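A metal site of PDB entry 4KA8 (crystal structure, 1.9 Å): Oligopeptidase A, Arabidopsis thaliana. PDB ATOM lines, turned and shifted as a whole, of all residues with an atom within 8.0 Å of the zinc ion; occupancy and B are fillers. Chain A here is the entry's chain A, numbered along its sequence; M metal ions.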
ATOM      1  N   ALA A 443      23.357 -17.996  10.474  1.00  0.00           N
ATOM      2  CA  ALA A 443      23.752 -17.923  11.881  1.00  0.00           C
ATOM      3  C   ALA A 443      24.275 -19.280  12.234  1.00  0.00           C
ATOM      4  O   ALA A 443      23.815 -20.299  11.666  1.00  0.00           O
ATOM      5  CB  ALA A 443      22.555 -17.533  12.764  1.00  0.00           C
ATOM      6  N   TRP A 444      25.297 -19.323  13.112  1.00  0.00           N
ATOM      7  CA  TRP A 444      25.884 -20.584  13.512  1.00  0.00           C
ATOM      8  C   TRP A 444      26.627 -20.458  14.841  1.00  0.00           C
ATOM      9  O   TRP A 444      26.850 -19.350  15.350  1.00  0.00           O
ATOM     10  CB  TRP A 444      26.838 -21.139  12.435  1.00  0.00           C
ATOM     11  CG  TRP A 444      28.108 -20.366  12.201  1.00  0.00           C
ATOM     12  CD1 TRP A 444      29.316 -20.615  12.756  1.00  0.00           C
ATOM     13  CD2 TRP A 444      28.276 -19.229  11.364  1.00  0.00           C
ATOM     14  NE1 TRP A 444      30.229 -19.692  12.340  1.00  0.00           N
ATOM     15  CE2 TRP A 444      29.622 -18.839  11.459  1.00  0.00           C
ATOM     16  CE3 TRP A 444      27.440 -18.527  10.489  1.00  0.00           C
ATOM     17  CZ2 TRP A 444      30.150 -17.766  10.749  1.00  0.00           C
ATOM     18  CZ3 TRP A 444      27.963 -17.439   9.785  1.00  0.00           C
ATOM     19  CH2 TRP A 444      29.307 -17.078   9.914  1.00  0.00           C
ATOM     20  N   MET A 445      26.996 -21.620  15.349  1.00  0.00           N
ATOM     21  CA  MET A 445      27.875 -21.775  16.493  1.00  0.00           C
ATOM     22  C   MET A 445      29.031 -22.625  16.043  1.00  0.00           C
ATOM     23  O   MET A 445      28.894 -23.574  15.222  1.00  0.00           O
ATOM     24  CB  MET A 445      27.125 -22.443  17.617  1.00  0.00           C
ATOM     25  CG  MET A 445      27.967 -22.853  18.822  1.00  0.00           C
ATOM     26  SD  MET A 445      28.677 -24.488  18.603  1.00  0.00           S
ATOM     27  CE  MET A 445      29.832 -24.500  19.984  1.00  0.00           C
ATOM     28  N   THR A 491      16.675 -16.691  16.772  1.00  0.00           N
ATOM     29  CA  THR A 491      17.981 -17.058  16.258  1.00  0.00           C
ATOM     30  C   THR A 491      19.086 -16.914  17.331  1.00  0.00           C
ATOM     31  O   THR A 491      19.922 -17.779  17.454  1.00  0.00           O
ATOM     32  CB  THR A 491      18.322 -16.267  14.998  1.00  0.00           C
ATOM     33  OG1 THR A 491      17.319 -16.558  14.018  1.00  0.00           O
ATOM     34  CG2 THR A 491      19.664 -16.647  14.468  1.00  0.00           C
ATOM     35  N   HIS A 494      18.656 -19.808  19.710  1.00  0.00           N
ATOM     36  CA  HIS A 494      19.106 -21.036  19.025  1.00  0.00           C
ATOM     37  C   HIS A 494      20.615 -21.239  19.099  1.00  0.00           C
ATOM     38  O   HIS A 494      21.099 -22.262  19.570  1.00  0.00           O
ATOM     39  CB  HIS A 494      18.664 -20.971  17.558  1.00  0.00           C
ATOM     40  CG  HIS A 494      19.028 -22.176  16.755  1.00  0.00           C
ATOM     41  ND1 HIS A 494      18.117 -23.173  16.473  1.00  0.00           N
ATOM     42  CD2 HIS A 494      20.203 -22.584  16.213  1.00  0.00           C
ATOM     43  CE1 HIS A 494      18.714 -24.131  15.792  1.00  0.00           C
ATOM     44  NE2 HIS A 494      19.990 -23.811  15.636  1.00  0.00           N
ATOM     45  N   GLU A 495      21.374 -20.258  18.670  1.00  0.00           N
ATOM     46  CA  GLU A 495      22.839 -20.378  18.659  1.00  0.00           C
ATOM     47  C   GLU A 495      23.373 -20.466  20.089  1.00  0.00           C
ATOM     48  O   GLU A 495      24.352 -21.152  20.338  1.00  0.00           O
ATOM     49  CB  GLU A 495      23.512 -19.213  17.920  1.00  0.00           C
ATOM     50  CG  GLU A 495      23.022 -18.986  16.472  1.00  0.00           C
ATOM     51  CD  GLU A 495      22.900 -20.263  15.636  1.00  0.00           C
ATOM     52  OE1 GLU A 495      23.654 -21.224  15.860  1.00  0.00           O
ATOM     53  OE2 GLU A 495      22.021 -20.307  14.752  1.00  0.00           O
ATOM     54  N   GLY A 497      21.847 -21.980  22.530  1.00  0.00           N
ATOM     55  CA  GLY A 497      21.645 -23.365  22.864  1.00  0.00           C
ATOM     56  C   GLY A 497      22.801 -24.273  22.513  1.00  0.00           C
ATOM     57  O   GLY A 497      23.214 -25.099  23.313  1.00  0.00           O
ATOM     58  N   HIS A 498      23.314 -24.161  21.294  1.00  0.00           N
ATOM     59  CA  HIS A 498      24.542 -24.870  20.926  1.00  0.00           C
ATOM     60  C   HIS A 498      25.726 -24.475  21.820  1.00  0.00           C
ATOM     61  O   HIS A 498      26.498 -25.339  22.255  1.00  0.00           O
ATOM     62  CB  HIS A 498      24.978 -24.464  19.531  1.00  0.00           C
ATOM     63  CG  HIS A 498      24.099 -24.962  18.431  1.00  0.00           C
ATOM     64  ND1 HIS A 498      23.764 -26.288  18.295  1.00  0.00           N
ATOM     65  CD2 HIS A 498      23.570 -24.327  17.358  1.00  0.00           C
ATOM     66  CE1 HIS A 498      23.020 -26.444  17.208  1.00  0.00           C
ATOM     67  NE2 HIS A 498      22.923 -25.273  16.614  1.00  0.00           N
ATOM     68  N   TRP A 520      24.797 -36.550  14.438  1.00  0.00           N
ATOM     69  CA  TRP A 520      24.416 -35.279  13.870  1.00  0.00           C
ATOM     70  C   TRP A 520      22.903 -34.982  13.938  1.00  0.00           C
ATOM     71  O   TRP A 520      22.512 -33.836  14.089  1.00  0.00           O
ATOM     72  CB  TRP A 520      24.943 -35.174  12.431  1.00  0.00           C
ATOM     73  CG  TRP A 520      24.994 -33.830  11.954  1.00  0.00           C
ATOM     74  CD1 TRP A 520      24.085 -33.209  11.139  1.00  0.00           C
ATOM     75  CD2 TRP A 520      25.975 -32.837  12.285  1.00  0.00           C
ATOM     76  NE1 TRP A 520      24.461 -31.908  10.922  1.00  0.00           N
ATOM     77  CE2 TRP A 520      25.615 -31.658  11.614  1.00  0.00           C
ATOM     78  CE3 TRP A 520      27.138 -32.848  13.071  1.00  0.00           C
ATOM     79  CZ2 TRP A 520      26.377 -30.471  11.701  1.00  0.00           C
ATOM     80  CZ3 TRP A 520      27.898 -31.670  13.161  1.00  0.00           C
ATOM     81  CH2 TRP A 520      27.511 -30.511  12.483  1.00  0.00           C
ATOM     82  N   VAL A 523      22.233 -33.006  17.314  1.00  0.00           N
ATOM     83  CA  VAL A 523      22.913 -31.750  17.682  1.00  0.00           C
ATOM     84  C   VAL A 523      21.998 -30.525  17.644  1.00  0.00           C
ATOM     85  O   VAL A 523      22.300 -29.512  18.278  1.00  0.00           O
ATOM     86  CB  VAL A 523      24.228 -31.492  16.901  1.00  0.00           C
ATOM     87  CG1 VAL A 523      25.040 -32.761  16.707  1.00  0.00           C
ATOM     88  CG2 VAL A 523      23.978 -30.760  15.587  1.00  0.00           C
ATOM     89  N   GLU A 524      20.852 -30.623  16.949  1.00  0.00           N
ATOM     90  CA  GLU A 524      19.871 -29.548  16.941  1.00  0.00           C
ATOM     91  C   GLU A 524      18.829 -29.633  18.080  1.00  0.00           C
ATOM     92  O   GLU A 524      17.834 -28.907  18.050  1.00  0.00           O
ATOM     93  CB  GLU A 524      19.190 -29.381  15.576  1.00  0.00           C
ATOM     94  CG  GLU A 524      20.151 -29.056  14.446  1.00  0.00           C
ATOM     95  CD  GLU A 524      20.846 -27.703  14.555  1.00  0.00           C
ATOM     96  OE1 GLU A 524      20.325 -26.734  15.168  1.00  0.00           O
ATOM     97  OE2 GLU A 524      21.945 -27.610  14.012  1.00  0.00           O
ATOM     98  N   LEU A 525      19.083 -30.465  19.078  1.00  0.00           N
ATOM     99  CA  LEU A 525      18.228 -30.581  20.257  1.00  0.00           C
ATOM    100  C   LEU A 525      18.316 -29.356  21.164  1.00  0.00           C
ATOM    101  O   LEU A 525      17.306 -28.695  21.338  1.00  0.00           O
ATOM    102  CB  LEU A 525      18.444 -31.917  21.012  1.00  0.00           C
ATOM    103  CG  LEU A 525      17.955 -32.158  22.459  1.00  0.00           C
ATOM    104  CD1 LEU A 525      16.546 -31.724  22.745  1.00  0.00           C
ATOM    105  CD2 LEU A 525      18.090 -33.640  22.828  1.00  0.00           C
ATOM    106  N   PRO A 526      19.509 -29.038  21.722  1.00  0.00           N
ATOM    107  CA  PRO A 526      19.520 -27.933  22.672  1.00  0.00           C
ATOM    108  C   PRO A 526      19.299 -26.540  22.051  1.00  0.00           C
ATOM    109  O   PRO A 526      18.764 -25.644  22.694  1.00  0.00           O
ATOM    110  CB  PRO A 526      20.928 -28.034  23.307  1.00  0.00           C
ATOM    111  CG  PRO A 526      21.748 -28.697  22.227  1.00  0.00           C
ATOM    112  CD  PRO A 526      20.807 -29.723  21.679  1.00  0.00           C
ATOM    113  N   SER A 527      19.663 -26.365  20.782  1.00  0.00           N
ATOM    114  CA  SER A 527      19.422 -25.098  20.113  1.00  0.00           C
ATOM    115  C   SER A 527      17.917 -24.846  19.921  1.00  0.00           C
ATOM    116  O   SER A 527      17.390 -23.831  20.354  1.00  0.00           O
ATOM    117  CB  SER A 527      20.217 -25.054  18.813  1.00  0.00           C
ATOM    118  OG  SER A 527      19.934 -26.241  18.063  1.00  0.00           O
ATOM    119  N   GLN A 528      17.204 -25.822  19.338  1.00  0.00           N
ATOM    120  CA  GLN A 528      15.777 -25.655  19.112  1.00  0.00           C
ATOM    121  C   GLN A 528      14.991 -25.637  20.432  1.00  0.00           C
ATOM    122  O   GLN A 528      13.995 -24.962  20.542  1.00  0.00           O
ATOM    123  CB  GLN A 528      15.271 -26.728  18.159  1.00  0.00           C
ATOM    124  CG  GLN A 528      15.802 -26.474  16.762  1.00  0.00           C
ATOM    125  CD  GLN A 528      15.411 -27.584  15.804  1.00  0.00           C
ATOM    126  OE1 GLN A 528      15.776 -28.759  15.989  1.00  0.00           O
ATOM    127  NE2 GLN A 528      14.681 -27.227  14.788  1.00  0.00           N
ATOM    128  N   GLU A 531      14.757 -22.027  21.871  1.00  0.00           N
ATOM    129  CA  GLU A 531      13.816 -21.163  21.172  1.00  0.00           C
ATOM    130  C   GLU A 531      12.389 -21.151  21.784  1.00  0.00           C
ATOM    131  O   GLU A 531      11.673 -20.152  21.668  1.00  0.00           O
ATOM    132  CB  GLU A 531      13.754 -21.532  19.667  1.00  0.00           C
ATOM    133  CG  GLU A 531      15.088 -21.621  18.933  1.00  0.00           C
ATOM    134  CD  GLU A 531      14.864 -21.856  17.432  1.00  0.00           C
ATOM    135  OE1 GLU A 531      14.000 -21.145  16.880  1.00  0.00           O
ATOM    136  OE2 GLU A 531      15.539 -22.715  16.815  1.00  0.00           O
ATOM    137  N   HIS A 626      24.126 -25.622   3.561  1.00  0.00           N
ATOM    138  CA  HIS A 626      23.945 -26.667   4.554  1.00  0.00           C
ATOM    139  C   HIS A 626      24.388 -28.058   4.030  1.00  0.00           C
ATOM    140  O   HIS A 626      25.076 -28.820   4.746  1.00  0.00           O
ATOM    141  CB  HIS A 626      22.456 -26.785   4.933  1.00  0.00           C
ATOM    142  CG  HIS A 626      22.009 -25.864   6.017  1.00  0.00           C
ATOM    143  ND1 HIS A 626      21.595 -24.574   5.792  1.00  0.00           N
ATOM    144  CD2 HIS A 626      21.882 -26.059   7.352  1.00  0.00           C
ATOM    145  CE1 HIS A 626      21.239 -24.013   6.929  1.00  0.00           C
ATOM    146  NE2 HIS A 626      21.389 -24.897   7.886  1.00  0.00           N
ATOM    147  N   TYR A 632      25.475 -31.049   6.738  1.00  0.00           N
ATOM    148  CA  TYR A 632      24.088 -31.575   6.616  1.00  0.00           C
ATOM    149  C   TYR A 632      23.805 -32.358   5.332  1.00  0.00           C
ATOM    150  O   TYR A 632      22.646 -32.580   5.016  1.00  0.00           O
ATOM    151  CB  TYR A 632      23.059 -30.429   6.780  1.00  0.00           C
ATOM    152  CG  TYR A 632      23.152 -29.728   8.122  1.00  0.00           C
ATOM    153  CD1 TYR A 632      24.144 -28.760   8.372  1.00  0.00           C
ATOM    154  CD2 TYR A 632      22.292 -30.047   9.157  1.00  0.00           C
ATOM    155  CE1 TYR A 632      24.240 -28.136   9.609  1.00  0.00           C
ATOM    156  CE2 TYR A 632      22.364 -29.397  10.391  1.00  0.00           C
ATOM    157  CZ  TYR A 632      23.354 -28.461  10.620  1.00  0.00           C
ATOM    158  OH  TYR A 632      23.432 -27.832  11.860  1.00  0.00           O
ATOM    159  N   TYR A 639      17.396 -31.430  11.545  1.00  0.00           N
ATOM    160  CA  TYR A 639      16.637 -30.381  12.235  1.00  0.00           C
ATOM    161  C   TYR A 639      15.302 -30.910  12.758  1.00  0.00           C
ATOM    162  O   TYR A 639      14.983 -30.759  13.960  1.00  0.00           O
ATOM    163  CB  TYR A 639      16.402 -29.153  11.348  1.00  0.00           C
ATOM    164  CG  TYR A 639      17.624 -28.266  11.150  1.00  0.00           C
ATOM    165  CD1 TYR A 639      18.016 -27.352  12.115  1.00  0.00           C
ATOM    166  CD2 TYR A 639      18.387 -28.359  10.007  1.00  0.00           C
ATOM    167  CE1 TYR A 639      19.130 -26.525  11.934  1.00  0.00           C
ATOM    168  CE2 TYR A 639      19.503 -27.559   9.814  1.00  0.00           C
ATOM    169  CZ  TYR A 639      19.875 -26.640  10.782  1.00  0.00           C
ATOM    170  OH  TYR A 639      20.970 -25.860  10.558  1.00  0.00           O
HETATM  171 ZN    ZN M   1      21.468 -25.144  15.005  1.00  0.00          ZN
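OE2 of Glu 524 is in hydrogen-bond range of OH of Tyr 632, 2.6 Å away. A ring nitrogen (NE2) of His 498 lies close to the side-chain hydroxyl (OG) of Ser 527 (3.5 Å). The side-chain carboxylate (OE2) of Glu 531 lies within hydrogen-bond range of a ring nitrogen (ND1) of His 494 (2.6 Å). OG of Ser 527 lies within hydrogen-bond range of O of Glu 524 (3.4 Å). A ring nitrogen (NE2) of His 494 sits close to the side-chain hydroxyl (OG) of Ser 527 (3.4 Å). The backbone carbonyl oxygen (O) of Glu 524 sits close to the side-chain amide oxygen (OE1) of Gln 528 (2.9 Å).
Merely in contact with the zinc ion: Ser 527. Four residues have an atom within 4 Å of the zinc ion: His 494, His 498, Glu 524 and Ser 527.
The zinc ion is bound by the side-chain carboxylate (OE1) of Glu 524 (2.0 Å), a ring nitrogen (NE2) of His 494 (2.1 Å) and a ring nitrogen (NE2) of His 498 (2.2 Å). The zinc ion has three donor atoms within binding distance. Slightly farther from the zinc ion lies OE2 of Glu 524 (2.7 Å).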
